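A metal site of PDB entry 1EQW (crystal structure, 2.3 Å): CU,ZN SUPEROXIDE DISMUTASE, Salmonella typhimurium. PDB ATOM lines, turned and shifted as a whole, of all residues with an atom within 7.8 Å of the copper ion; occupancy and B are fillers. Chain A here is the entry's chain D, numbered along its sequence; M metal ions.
A ring nitrogen (ND1) of His 129 is in hydrogen-bond range of the backbone carbonyl oxygen (O) of Gly 146 (3.0 Å). The backbone NH of His 129 lies within hydrogen-bond range of the backbone carbonyl oxygen of Gly 46 (2.9 Å). O of Ser 125 sits at hydrogen-bond distance from N of His 50, 2.7 Å away. O of His 48 is in hydrogen-bond range of N of Met 127 (2.7 Å). A ring nitrogen (ND1) of His 50 sits at hydrogen-bond distance from the backbone carbonyl oxygen (O) of Gly 71, 3.0 Å away. A ring nitrogen (ND1) of His 129 sits close to the backbone carbonyl oxygen (O) of Ala 147 (3.4 Å). A ring nitrogen (NE2) of His 48 lies within hydrogen-bond range of the side-chain carboxylate (OD2) of Asp 133, 2.6 Å away.
His 73 touches the copper ion (NE2 to CU, 3.2 Å). Of the 24 residues printed, 4 come within 4 Å of the copper ion. The nearest printed residue that does not touch the copper ion is Met 127 (4.1 Å).
The copper ion is bound by a ring nitrogen (NE2) of His 129 (2.0 Å), a ring nitrogen (ND1) of His 48 (2.0 Å) and a ring nitrogen (NE2) of His 50 (2.2 Å). The copper ion has three donor atoms within binding distance.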
ATOM      1  N   GLY A  46      13.859  11.930 -13.479  1.00  0.00           N
ATOM      2  CA  GLY A  46      13.252  12.173 -14.775  1.00  0.00           C
ATOM      3  C   GLY A  46      12.549  10.883 -15.140  1.00  0.00           C
ATOM      4  O   GLY A  46      13.110   9.802 -14.975  1.00  0.00           O
ATOM      5  N   PHE A  47      11.327  11.017 -15.632  1.00  0.00           N
ATOM      6  CA  PHE A  47      10.527   9.851 -16.011  1.00  0.00           C
ATOM      7  C   PHE A  47       9.823  10.099 -17.327  1.00  0.00           C
ATOM      8  O   PHE A  47       8.878  10.897 -17.371  1.00  0.00           O
ATOM      9  CB  PHE A  47       9.510   9.564 -14.909  1.00  0.00           C
ATOM     10  CG  PHE A  47       8.612   8.402 -15.088  1.00  0.00           C
ATOM     11  CD1 PHE A  47       9.072   7.170 -15.518  1.00  0.00           C
ATOM     12  CD2 PHE A  47       7.251   8.545 -14.800  1.00  0.00           C
ATOM     13  CE1 PHE A  47       8.210   6.093 -15.659  1.00  0.00           C
ATOM     14  CE2 PHE A  47       6.386   7.477 -14.936  1.00  0.00           C
ATOM     15  CZ  PHE A  47       6.859   6.240 -15.371  1.00  0.00           C
ATOM     16  N   HIS A  48      10.258   9.441 -18.402  1.00  0.00           N
ATOM     17  CA  HIS A  48       9.619   9.654 -19.707  1.00  0.00           C
ATOM     18  C   HIS A  48       9.451   8.411 -20.542  1.00  0.00           C
ATOM     19  O   HIS A  48      10.121   7.391 -20.300  1.00  0.00           O
ATOM     20  CB  HIS A  48      10.417  10.635 -20.567  1.00  0.00           C
ATOM     21  CG  HIS A  48      11.280  11.613 -19.734  1.00  0.00           C
ATOM     22  ND1 HIS A  48      12.648  11.504 -19.600  1.00  0.00           N
ATOM     23  CD2 HIS A  48      10.912  12.706 -19.031  1.00  0.00           C
ATOM     24  CE1 HIS A  48      13.092  12.491 -18.840  1.00  0.00           C
ATOM     25  NE2 HIS A  48      12.053  13.241 -18.481  1.00  0.00           N
ATOM     26  N   VAL A  49       8.552   8.500 -21.505  1.00  0.00           N
ATOM     27  CA  VAL A  49       8.305   7.438 -22.455  1.00  0.00           C
ATOM     28  C   VAL A  49       9.258   7.661 -23.624  1.00  0.00           C
ATOM     29  O   VAL A  49       9.279   8.749 -24.211  1.00  0.00           O
ATOM     30  CB  VAL A  49       6.869   7.512 -23.000  1.00  0.00           C
ATOM     31  CG1 VAL A  49       6.609   6.365 -23.959  1.00  0.00           C
ATOM     32  CG2 VAL A  49       5.870   7.513 -21.862  1.00  0.00           C
ATOM     33  N   HIS A  50      10.076   6.662 -23.951  1.00  0.00           N
ATOM     34  CA  HIS A  50      10.995   6.802 -25.064  1.00  0.00           C
ATOM     35  C   HIS A  50      10.482   6.048 -26.296  1.00  0.00           C
ATOM     36  O   HIS A  50       9.690   5.106 -26.184  1.00  0.00           O
ATOM     37  CB  HIS A  50      12.378   6.311 -24.699  1.00  0.00           C
ATOM     38  CG  HIS A  50      13.127   7.322 -23.800  1.00  0.00           C
ATOM     39  ND1 HIS A  50      14.402   7.764 -24.075  1.00  0.00           N
ATOM     40  CD2 HIS A  50      12.748   7.947 -22.663  1.00  0.00           C
ATOM     41  CE1 HIS A  50      14.782   8.622 -23.139  1.00  0.00           C
ATOM     42  NE2 HIS A  50      13.792   8.746 -22.273  1.00  0.00           N
ATOM     43  N   GLY A  71      16.386   5.288 -27.835  1.00  0.00           N
ATOM     44  CA  GLY A  71      16.122   6.470 -28.641  1.00  0.00           C
ATOM     45  C   GLY A  71      15.747   7.688 -27.810  1.00  0.00           C
ATOM     46  O   GLY A  71      16.017   7.735 -26.604  1.00  0.00           O
ATOM     47  N   GLY A  72      15.135   8.673 -28.457  1.00  0.00           N
ATOM     48  CA  GLY A  72      14.725   9.885 -27.772  1.00  0.00           C
ATOM     49  C   GLY A  72      13.361   9.709 -27.167  1.00  0.00           C
ATOM     50  O   GLY A  72      12.826   8.595 -27.139  1.00  0.00           O
ATOM     51  N   HIS A  73      12.790  10.810 -26.680  1.00  0.00           N
ATOM     52  CA  HIS A  73      11.474  10.802 -26.065  1.00  0.00           C
ATOM     53  C   HIS A  73      10.375  10.696 -27.111  1.00  0.00           C
ATOM     54  O   HIS A  73      10.497  11.245 -28.212  1.00  0.00           O
ATOM     55  CB  HIS A  73      11.230  12.071 -25.249  1.00  0.00           C
ATOM     56  CG  HIS A  73      12.329  12.359 -24.242  1.00  0.00           C
ATOM     57  ND1 HIS A  73      12.299  13.443 -23.390  1.00  0.00           N
ATOM     58  CD2 HIS A  73      13.480  11.700 -23.962  1.00  0.00           C
ATOM     59  CE1 HIS A  73      13.381  13.441 -22.631  1.00  0.00           C
ATOM     60  NE2 HIS A  73      14.112  12.388 -22.956  1.00  0.00           N
ATOM     61  N   LEU A  74       9.299   9.991 -26.781  1.00  0.00           N
ATOM     62  CA  LEU A  74       8.174   9.819 -27.694  1.00  0.00           C
ATOM     63  C   LEU A  74       7.636  11.168 -28.125  1.00  0.00           C
ATOM     64  O   LEU A  74       7.011  11.882 -27.335  1.00  0.00           O
ATOM     65  CB  LEU A  74       7.061   8.987 -27.040  1.00  0.00           C
ATOM     66  CG  LEU A  74       5.781   8.879 -27.860  1.00  0.00           C
ATOM     67  CD1 LEU A  74       6.015   8.046 -29.111  1.00  0.00           C
ATOM     68  CD2 LEU A  74       4.645   8.287 -27.035  1.00  0.00           C
ATOM     69  N   HIS A  82      11.088  19.852 -25.082  1.00  0.00           N
ATOM     70  CA  HIS A  82      10.823  19.154 -23.832  1.00  0.00           C
ATOM     71  C   HIS A  82      10.093  20.128 -22.888  1.00  0.00           C
ATOM     72  O   HIS A  82      10.727  20.977 -22.260  1.00  0.00           O
ATOM     73  CB  HIS A  82      12.143  18.690 -23.229  1.00  0.00           C
ATOM     74  CG  HIS A  82      11.959  17.916 -21.934  1.00  0.00           C
ATOM     75  ND1 HIS A  82      11.285  16.716 -21.897  1.00  0.00           N
ATOM     76  CD2 HIS A  82      12.338  18.176 -20.661  1.00  0.00           C
ATOM     77  CE1 HIS A  82      11.265  16.258 -20.654  1.00  0.00           C
ATOM     78  NE2 HIS A  82      11.897  17.129 -19.885  1.00  0.00           N
ATOM     79  N   HIS A  91       7.493  17.133 -26.123  1.00  0.00           N
ATOM     80  CA  HIS A  91       7.449  15.685 -26.227  1.00  0.00           C
ATOM     81  C   HIS A  91       6.223  15.092 -25.545  1.00  0.00           C
ATOM     82  O   HIS A  91       5.996  15.315 -24.348  1.00  0.00           O
ATOM     83  CB  HIS A  91       8.691  15.051 -25.605  1.00  0.00           C
ATOM     84  CG  HIS A  91       9.989  15.674 -26.102  1.00  0.00           C
ATOM     85  ND1 HIS A  91      11.174  15.613 -25.411  1.00  0.00           N
ATOM     86  CD2 HIS A  91      10.264  16.359 -27.245  1.00  0.00           C
ATOM     87  CE1 HIS A  91      12.129  16.226 -26.088  1.00  0.00           C
ATOM     88  NE2 HIS A  91      11.592  16.688 -27.211  1.00  0.00           N
ATOM     89  N   GLY A  93       5.838  12.172 -24.744  1.00  0.00           N
ATOM     90  CA  GLY A  93       6.305  11.154 -23.803  1.00  0.00           C
ATOM     91  C   GLY A  93       6.750  11.724 -22.446  1.00  0.00           C
ATOM     92  O   GLY A  93       7.202  10.986 -21.570  1.00  0.00           O
ATOM     93  N   ASP A  94       6.616  13.024 -22.254  1.00  0.00           N
ATOM     94  CA  ASP A  94       7.022  13.663 -20.989  1.00  0.00           C
ATOM     95  C   ASP A  94       6.036  13.380 -19.857  1.00  0.00           C
ATOM     96  O   ASP A  94       4.920  13.883 -19.847  1.00  0.00           O
ATOM     97  CB  ASP A  94       7.171  15.168 -21.180  1.00  0.00           C
ATOM     98  CG  ASP A  94       8.396  15.537 -21.972  1.00  0.00           C
ATOM     99  OD1 ASP A  94       9.144  14.610 -22.372  1.00  0.00           O
ATOM    100  OD2 ASP A  94       8.625  16.745 -22.193  1.00  0.00           O
ATOM    101  N   SER A 125       8.947   2.546 -24.674  1.00  0.00           N
ATOM    102  CA  SER A 125       9.575   2.177 -23.418  1.00  0.00           C
ATOM    103  C   SER A 125       9.450   3.255 -22.349  1.00  0.00           C
ATOM    104  O   SER A 125       9.221   4.427 -22.669  1.00  0.00           O
ATOM    105  CB  SER A 125      11.059   1.865 -23.665  1.00  0.00           C
ATOM    106  OG  SER A 125      11.670   2.879 -24.439  1.00  0.00           O
ATOM    107  N   LEU A 126       9.579   2.856 -21.085  1.00  0.00           N
ATOM    108  CA  LEU A 126       9.498   3.784 -19.969  1.00  0.00           C
ATOM    109  C   LEU A 126      10.920   3.967 -19.432  1.00  0.00           C
ATOM    110  O   LEU A 126      11.636   2.993 -19.222  1.00  0.00           O
ATOM    111  CB  LEU A 126       8.587   3.253 -18.850  1.00  0.00           C
ATOM    112  CG  LEU A 126       7.125   3.021 -19.229  1.00  0.00           C
ATOM    113  CD1 LEU A 126       6.326   2.546 -18.025  1.00  0.00           C
ATOM    114  CD2 LEU A 126       6.503   4.290 -19.789  1.00  0.00           C
ATOM    115  N   MET A 127      11.315   5.209 -19.208  1.00  0.00           N
ATOM    116  CA  MET A 127      12.670   5.486 -18.721  1.00  0.00           C
ATOM    117  C   MET A 127      12.729   6.248 -17.402  1.00  0.00           C
ATOM    118  O   MET A 127      11.943   7.174 -17.157  1.00  0.00           O
ATOM    119  CB  MET A 127      13.427   6.255 -19.791  1.00  0.00           C
ATOM    120  CG  MET A 127      14.940   6.217 -19.640  1.00  0.00           C
ATOM    121  SD  MET A 127      15.685   4.863 -20.573  1.00  0.00           S
ATOM    122  CE  MET A 127      16.611   4.034 -19.287  1.00  0.00           C
ATOM    123  N   ILE A 128      13.677   5.848 -16.561  1.00  0.00           N
ATOM    124  CA  ILE A 128      13.918   6.510 -15.281  1.00  0.00           C
ATOM    125  C   ILE A 128      15.371   6.954 -15.330  1.00  0.00           C
ATOM    126  O   ILE A 128      16.284   6.141 -15.415  1.00  0.00           O
ATOM    127  CB  ILE A 128      13.732   5.544 -14.090  1.00  0.00           C
ATOM    128  CG1 ILE A 128      12.284   5.052 -14.022  1.00  0.00           C
ATOM    129  CG2 ILE A 128      14.115   6.224 -12.787  1.00  0.00           C
ATOM    130  CD1 ILE A 128      11.951   4.310 -12.757  1.00  0.00           C
ATOM    131  N   HIS A 129      15.574   8.272 -15.287  1.00  0.00           N
ATOM    132  CA  HIS A 129      16.925   8.830 -15.355  1.00  0.00           C
ATOM    133  C   HIS A 129      17.567   9.012 -13.999  1.00  0.00           C
ATOM    134  O   HIS A 129      16.927   8.850 -12.963  1.00  0.00           O
ATOM    135  CB  HIS A 129      16.878  10.195 -16.030  1.00  0.00           C
ATOM    136  CG  HIS A 129      16.422  10.103 -17.497  1.00  0.00           C
ATOM    137  ND1 HIS A 129      17.284  10.140 -18.571  1.00  0.00           N
ATOM    138  CD2 HIS A 129      15.174  10.002 -18.017  1.00  0.00           C
ATOM    139  CE1 HIS A 129      16.593  10.066 -19.694  1.00  0.00           C
ATOM    140  NE2 HIS A 129      15.313   9.980 -19.386  1.00  0.00           N
ATOM    141  N   ASP A 133      13.902  16.532 -13.157  1.00  0.00           N
ATOM    142  CA  ASP A 133      13.189  17.037 -14.321  1.00  0.00           C
ATOM    143  C   ASP A 133      12.455  18.344 -13.996  1.00  0.00           C
ATOM    144  O   ASP A 133      11.502  18.349 -13.215  1.00  0.00           O
ATOM    145  CB  ASP A 133      12.198  15.984 -14.803  1.00  0.00           C
ATOM    146  CG  ASP A 133      11.713  16.196 -16.225  1.00  0.00           C
ATOM    147  OD1 ASP A 133      11.720  17.342 -16.695  1.00  0.00           O
ATOM    148  OD2 ASP A 133      11.332  15.194 -16.868  1.00  0.00           O
ATOM    149  N   LEU A 142      16.598  18.608 -21.785  1.00  0.00           N
ATOM    150  CA  LEU A 142      15.710  17.518 -21.406  1.00  0.00           C
ATOM    151  C   LEU A 142      15.421  17.470 -19.901  1.00  0.00           C
ATOM    152  O   LEU A 142      15.301  16.392 -19.321  1.00  0.00           O
ATOM    153  CB  LEU A 142      16.302  16.177 -21.866  1.00  0.00           C
ATOM    154  N   GLY A 145      17.697  15.392 -16.982  1.00  0.00           N
ATOM    155  CA  GLY A 145      17.526  14.013 -16.554  1.00  0.00           C
ATOM    156  C   GLY A 145      18.842  13.279 -16.480  1.00  0.00           C
ATOM    157  O   GLY A 145      19.049  12.423 -15.600  1.00  0.00           O
ATOM    158  N   GLY A 146      19.750  13.600 -17.399  1.00  0.00           N
ATOM    159  CA  GLY A 146      21.048  12.966 -17.418  1.00  0.00           C
ATOM    160  C   GLY A 146      20.981  11.515 -17.844  1.00  0.00           C
ATOM    161  O   GLY A 146      20.091  11.114 -18.599  1.00  0.00           O
ATOM    162  N   ALA A 147      21.920  10.730 -17.350  1.00  0.00           N
ATOM    163  CA  ALA A 147      22.008   9.304 -17.659  1.00  0.00           C
ATOM    164  C   ALA A 147      20.720   8.530 -17.386  1.00  0.00           C
ATOM    165  O   ALA A 147      19.861   8.966 -16.624  1.00  0.00           O
ATOM    166  CB  ALA A 147      23.142   8.664 -16.887  1.00  0.00           C
ATOM    167  N   ARG A 148      20.616   7.371 -18.028  1.00  0.00           N
ATOM    168  CA  ARG A 148      19.479   6.479 -17.901  1.00  0.00           C
ATOM    169  C   ARG A 148      19.805   5.424 -16.854  1.00  0.00           C
ATOM    170  O   ARG A 148      20.779   4.673 -16.989  1.00  0.00           O
ATOM    171  CB  ARG A 148      19.107   5.857 -19.234  1.00  0.00           C
ATOM    172  CG  ARG A 148      19.037   6.931 -20.318  1.00  0.00           C
ATOM    173  CD  ARG A 148      18.819   6.405 -21.727  1.00  0.00           C
ATOM    174  NE  ARG A 148      18.661   7.544 -22.627  1.00  0.00           N
ATOM    175  CZ  ARG A 148      18.260   7.472 -23.898  1.00  0.00           C
ATOM    176  NH1 ARG A 148      17.963   6.301 -24.443  1.00  0.00           N
ATOM    177  NH2 ARG A 148      18.147   8.597 -24.595  1.00  0.00           N
HETATM  178 CU    CU M   1      13.834  10.209 -20.638  1.00  0.00          CU
HETATM  179 ZN    ZN M   2      10.854  15.197 -23.169  1.00  0.00          ZN
